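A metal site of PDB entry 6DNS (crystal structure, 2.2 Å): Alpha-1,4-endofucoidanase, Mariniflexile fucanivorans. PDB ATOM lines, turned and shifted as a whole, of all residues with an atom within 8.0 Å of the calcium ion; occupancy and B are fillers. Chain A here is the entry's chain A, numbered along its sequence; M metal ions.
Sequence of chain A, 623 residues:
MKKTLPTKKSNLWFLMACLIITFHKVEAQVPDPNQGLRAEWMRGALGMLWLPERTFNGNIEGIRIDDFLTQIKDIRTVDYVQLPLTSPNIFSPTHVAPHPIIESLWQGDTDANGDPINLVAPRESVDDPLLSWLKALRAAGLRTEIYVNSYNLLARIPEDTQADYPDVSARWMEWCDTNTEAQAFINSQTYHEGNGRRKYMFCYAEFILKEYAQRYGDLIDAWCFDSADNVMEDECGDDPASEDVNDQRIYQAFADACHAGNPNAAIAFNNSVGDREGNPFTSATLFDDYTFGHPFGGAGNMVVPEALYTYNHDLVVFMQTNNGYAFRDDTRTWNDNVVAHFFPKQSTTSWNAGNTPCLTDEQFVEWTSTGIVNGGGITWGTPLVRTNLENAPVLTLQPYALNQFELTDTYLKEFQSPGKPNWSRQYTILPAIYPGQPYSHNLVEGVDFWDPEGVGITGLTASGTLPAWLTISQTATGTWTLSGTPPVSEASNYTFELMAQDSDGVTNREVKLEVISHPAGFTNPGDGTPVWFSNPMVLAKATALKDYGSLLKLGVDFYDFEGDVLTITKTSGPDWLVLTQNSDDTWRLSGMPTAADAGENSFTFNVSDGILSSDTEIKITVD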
ATOM      1  N   GLN A 437      -7.772  35.538  32.289  1.00  0.00           N
ATOM      2  CA  GLN A 437      -8.900  35.428  31.372  1.00  0.00           C
ATOM      3  C   GLN A 437     -10.081  36.270  31.872  1.00  0.00           C
ATOM      4  O   GLN A 437     -10.163  36.544  33.069  1.00  0.00           O
ATOM      5  CB  GLN A 437      -9.358  33.970  31.234  1.00  0.00           C
ATOM      6  CG  GLN A 437      -8.244  32.976  30.885  1.00  0.00           C
ATOM      7  CD  GLN A 437      -7.531  33.322  29.588  1.00  0.00           C
ATOM      8  OE1 GLN A 437      -8.171  33.575  28.566  1.00  0.00           O
ATOM      9  NE2 GLN A 437      -6.207  33.320  29.633  1.00  0.00           N
ATOM     10  N   ASP A 527      -2.706  30.473  23.314  1.00  0.00           N
ATOM     11  CA  ASP A 527      -3.437  31.122  22.208  1.00  0.00           C
ATOM     12  C   ASP A 527      -4.934  30.740  22.135  1.00  0.00           C
ATOM     13  O   ASP A 527      -5.581  31.000  21.116  1.00  0.00           O
ATOM     14  CB  ASP A 527      -2.729  30.824  20.875  1.00  0.00           C
ATOM     15  CG  ASP A 527      -2.659  29.326  20.543  1.00  0.00           C
ATOM     16  OD1 ASP A 527      -3.034  28.487  21.386  1.00  0.00           O
ATOM     17  OD2 ASP A 527      -2.225  28.997  19.422  1.00  0.00           O
ATOM     18  N   GLY A 528      -5.477  30.159  23.200  1.00  0.00           N
ATOM     19  CA  GLY A 528      -6.855  29.665  23.217  1.00  0.00           C
ATOM     20  C   GLY A 528      -7.087  28.260  22.671  1.00  0.00           C
ATOM     21  O   GLY A 528      -8.214  27.771  22.731  1.00  0.00           O
ATOM     22  N   THR A 529      -6.039  27.595  22.174  1.00  0.00           N
ATOM     23  CA  THR A 529      -6.191  26.321  21.482  1.00  0.00           C
ATOM     24  C   THR A 529      -6.428  25.172  22.468  1.00  0.00           C
ATOM     25  O   THR A 529      -5.634  24.988  23.389  1.00  0.00           O
ATOM     26  CB  THR A 529      -4.951  25.988  20.618  1.00  0.00           C
ATOM     27  OG1 THR A 529      -4.728  27.042  19.678  1.00  0.00           O
ATOM     28  CG2 THR A 529      -5.127  24.673  19.860  1.00  0.00           C
ATOM     29  N   PRO A 530      -7.519  24.398  22.292  1.00  0.00           N
ATOM     30  CA  PRO A 530      -7.687  23.176  23.088  1.00  0.00           C
ATOM     31  C   PRO A 530      -6.775  22.072  22.568  1.00  0.00           C
ATOM     32  O   PRO A 530      -6.662  21.886  21.351  1.00  0.00           O
ATOM     33  CB  PRO A 530      -9.162  22.815  22.879  1.00  0.00           C
ATOM     34  CG  PRO A 530      -9.494  23.370  21.530  1.00  0.00           C
ATOM     35  CD  PRO A 530      -8.631  24.580  21.333  1.00  0.00           C
ATOM     36  N   VAL A 531      -6.148  21.334  23.487  1.00  0.00           N
ATOM     37  CA  VAL A 531      -5.074  20.400  23.144  1.00  0.00           C
ATOM     38  C   VAL A 531      -5.336  18.988  23.661  1.00  0.00           C
ATOM     39  O   VAL A 531      -5.958  18.800  24.712  1.00  0.00           O
ATOM     40  CB  VAL A 531      -3.694  20.891  23.662  1.00  0.00           C
ATOM     41  CG1 VAL A 531      -3.311  22.197  22.988  1.00  0.00           C
ATOM     42  CG2 VAL A 531      -3.681  21.063  25.185  1.00  0.00           C
ATOM     43  N   TYR A 559      -7.755  18.601  26.948  1.00  0.00           N
ATOM     44  CA  TYR A 559      -7.971  19.716  27.875  1.00  0.00           C
ATOM     45  C   TYR A 559      -7.972  21.081  27.180  1.00  0.00           C
ATOM     46  O   TYR A 559      -7.336  21.261  26.144  1.00  0.00           O
ATOM     47  CB  TYR A 559      -6.920  19.700  29.002  1.00  0.00           C
ATOM     48  CG  TYR A 559      -7.182  20.706  30.104  1.00  0.00           C
ATOM     49  CD1 TYR A 559      -8.287  20.573  30.937  1.00  0.00           C
ATOM     50  CD2 TYR A 559      -6.331  21.792  30.306  1.00  0.00           C
ATOM     51  CE1 TYR A 559      -8.547  21.498  31.951  1.00  0.00           C
ATOM     52  CE2 TYR A 559      -6.578  22.717  31.315  1.00  0.00           C
ATOM     53  CZ  TYR A 559      -7.683  22.564  32.125  1.00  0.00           C
ATOM     54  OH  TYR A 559      -7.929  23.476  33.133  1.00  0.00           O
ATOM     55  N   ASP A 560      -8.715  22.013  27.770  1.00  0.00           N
ATOM     56  CA  ASP A 560      -8.740  23.413  27.353  1.00  0.00           C
ATOM     57  C   ASP A 560      -8.441  24.295  28.568  1.00  0.00           C
ATOM     58  O   ASP A 560      -9.097  24.170  29.602  1.00  0.00           O
ATOM     59  CB  ASP A 560     -10.115  23.769  26.790  1.00  0.00           C
ATOM     60  CG  ASP A 560     -10.174  25.167  26.225  1.00  0.00           C
ATOM     61  OD1 ASP A 560     -10.836  26.039  26.836  1.00  0.00           O
ATOM     62  OD2 ASP A 560      -9.553  25.419  25.165  1.00  0.00           O
ATOM     63  N   PHE A 561      -7.455  25.184  28.434  1.00  0.00           N
ATOM     64  CA  PHE A 561      -6.974  25.995  29.555  1.00  0.00           C
ATOM     65  C   PHE A 561      -7.863  27.200  29.897  1.00  0.00           C
ATOM     66  O   PHE A 561      -7.680  27.814  30.957  1.00  0.00           O
ATOM     67  CB  PHE A 561      -5.526  26.445  29.316  1.00  0.00           C
ATOM     68  CG  PHE A 561      -4.530  25.324  29.428  1.00  0.00           C
ATOM     69  CD1 PHE A 561      -4.308  24.456  28.365  1.00  0.00           C
ATOM     70  CD2 PHE A 561      -3.815  25.124  30.615  1.00  0.00           C
ATOM     71  CE1 PHE A 561      -3.392  23.416  28.478  1.00  0.00           C
ATOM     72  CE2 PHE A 561      -2.899  24.084  30.728  1.00  0.00           C
ATOM     73  CZ  PHE A 561      -2.688  23.222  29.659  1.00  0.00           C
ATOM     74  N   GLU A 562      -8.805  27.544  29.015  1.00  0.00           N
ATOM     75  CA  GLU A 562      -9.801  28.605  29.288  1.00  0.00           C
ATOM     76  C   GLU A 562     -11.106  28.033  29.876  1.00  0.00           C
ATOM     77  O   GLU A 562     -11.968  28.804  30.304  1.00  0.00           O
ATOM     78  CB  GLU A 562     -10.114  29.405  28.013  1.00  0.00           C
ATOM     79  CG  GLU A 562      -8.985  30.297  27.523  1.00  0.00           C
ATOM     80  CD  GLU A 562      -7.807  29.537  26.930  1.00  0.00           C
ATOM     81  OE1 GLU A 562      -8.012  28.462  26.317  1.00  0.00           O
ATOM     82  OE2 GLU A 562      -6.667  30.009  27.079  1.00  0.00           O
ATOM     83  N   GLY A 563     -11.247  26.714  29.876  1.00  0.00           N
ATOM     84  CA  GLY A 563     -12.473  26.059  30.356  1.00  0.00           C
ATOM     85  C   GLY A 563     -13.638  26.176  29.384  1.00  0.00           C
ATOM     86  O   GLY A 563     -14.800  26.129  29.811  1.00  0.00           O
ATOM     87  N   ASP A 564     -13.347  26.300  28.094  1.00  0.00           N
ATOM     88  CA  ASP A 564     -14.389  26.376  27.062  1.00  0.00           C
ATOM     89  C   ASP A 564     -14.975  24.979  26.858  1.00  0.00           C
ATOM     90  O   ASP A 564     -14.245  23.989  26.894  1.00  0.00           O
ATOM     91  CB  ASP A 564     -13.830  26.892  25.732  1.00  0.00           C
ATOM     92  CG  ASP A 564     -13.270  28.307  25.830  1.00  0.00           C
ATOM     93  OD1 ASP A 564     -13.756  29.109  26.649  1.00  0.00           O
ATOM     94  OD2 ASP A 564     -12.327  28.620  25.064  1.00  0.00           O
ATOM     95  N   VAL A 565     -16.286  24.910  26.656  1.00  0.00           N
ATOM     96  CA  VAL A 565     -16.964  23.648  26.340  1.00  0.00           C
ATOM     97  C   VAL A 565     -16.452  23.134  24.992  1.00  0.00           C
ATOM     98  O   VAL A 565     -16.260  23.911  24.057  1.00  0.00           O
ATOM     99  CB  VAL A 565     -18.507  23.783  26.362  1.00  0.00           C
ATOM    100  CG1 VAL A 565     -19.026  24.610  25.189  1.00  0.00           C
ATOM    101  CG2 VAL A 565     -19.165  22.407  26.389  1.00  0.00           C
ATOM    102  N   LEU A 566     -16.225  21.818  24.903  1.00  0.00           N
ATOM    103  CA  LEU A 566     -15.509  21.228  23.775  1.00  0.00           C
ATOM    104  C   LEU A 566     -16.332  20.243  22.953  1.00  0.00           C
ATOM    105  O   LEU A 566     -17.309  19.678  23.447  1.00  0.00           O
ATOM    106  CB  LEU A 566     -14.232  20.544  24.261  1.00  0.00           C
ATOM    107  CG  LEU A 566     -13.280  21.393  25.114  1.00  0.00           C
ATOM    108  CD1 LEU A 566     -12.067  20.567  25.525  1.00  0.00           C
ATOM    109  CD2 LEU A 566     -12.849  22.661  24.399  1.00  0.00           C
ATOM    110  N   SER A 608     -12.220  20.866  19.434  1.00  0.00           N
ATOM    111  CA  SER A 608     -12.536  22.267  19.109  1.00  0.00           C
ATOM    112  C   SER A 608     -13.262  22.977  20.255  1.00  0.00           C
ATOM    113  O   SER A 608     -13.691  22.336  21.210  1.00  0.00           O
ATOM    114  CB  SER A 608     -13.405  22.307  17.848  1.00  0.00           C
ATOM    115  OG  SER A 608     -13.723  23.640  17.468  1.00  0.00           O
ATOM    116  N   ASP A 609     -13.395  24.301  20.136  1.00  0.00           N
ATOM    117  CA  ASP A 609     -14.158  25.117  21.085  1.00  0.00           C
ATOM    118  C   ASP A 609     -15.106  26.090  20.382  1.00  0.00           C
ATOM    119  O   ASP A 609     -15.290  26.030  19.165  1.00  0.00           O
ATOM    120  CB  ASP A 609     -13.234  25.880  22.065  1.00  0.00           C
ATOM    121  CG  ASP A 609     -12.162  26.728  21.360  1.00  0.00           C
ATOM    122  OD1 ASP A 609     -12.321  27.065  20.164  1.00  0.00           O
ATOM    123  OD2 ASP A 609     -11.157  27.064  22.019  1.00  0.00           O
ATOM    124  N   ILE A 611     -13.912  27.774  17.526  1.00  0.00           N
ATOM    125  CA  ILE A 611     -13.027  28.657  16.776  1.00  0.00           C
ATOM    126  C   ILE A 611     -11.663  27.988  16.564  1.00  0.00           C
ATOM    127  O   ILE A 611     -11.333  27.611  15.440  1.00  0.00           O
ATOM    128  CB  ILE A 611     -12.851  30.009  17.482  1.00  0.00           C
ATOM    129  N   LEU A 612     -10.888  27.853  17.644  1.00  0.00           N
ATOM    130  CA  LEU A 612      -9.568  27.211  17.578  1.00  0.00           C
ATOM    131  C   LEU A 612      -9.700  25.700  17.763  1.00  0.00           C
ATOM    132  O   LEU A 612     -10.614  25.236  18.460  1.00  0.00           O
ATOM    133  CB  LEU A 612      -8.642  27.786  18.649  1.00  0.00           C
ATOM    134  N   SER A 613      -8.811  24.940  17.132  1.00  0.00           N
ATOM    135  CA  SER A 613      -8.811  23.482  17.235  1.00  0.00           C
ATOM    136  C   SER A 613      -7.444  22.869  16.905  1.00  0.00           C
ATOM    137  O   SER A 613      -6.564  23.543  16.377  1.00  0.00           O
ATOM    138  CB  SER A 613      -9.882  22.871  16.315  1.00  0.00           C
ATOM    139  OG  SER A 613      -9.646  23.180  14.955  1.00  0.00           O
HETATM  140 CA    CA M   1     -10.150  27.904  24.214  1.00  0.00          CA
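Along chain A the residues within 4 Å of the calcium ion span positions 528 to 609.
The calcium ion is bound by the backbone carbonyl oxygen of Gly 528 (2.4 Å), the side-chain carboxylate of Asp 564 (2.4 Å), the side-chain carboxylate of Asp 609 (2.6 Å) and the side-chain carboxylate of Asp 560 (2.7 Å). The calcium ion has four donor atoms within binding distance. Slightly farther from the calcium ion lies OE1 of Glu 562 (3.1 Å).
The side-chain carboxylate (OD1) of Asp 609 sits at hydrogen-bond distance from the backbone NH (N) of Ile 611 (3.2 Å). OD1 of Asp 609 sits at hydrogen-bond distance from N of Leu 612 (3.0 Å). N of Glu 562 sits close to OD1 of Asp 560 (3.3 Å). The backbone NH of Gly 563 sits at hydrogen-bond distance from the side-chain carboxylate of Asp 560 (3.1 Å).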
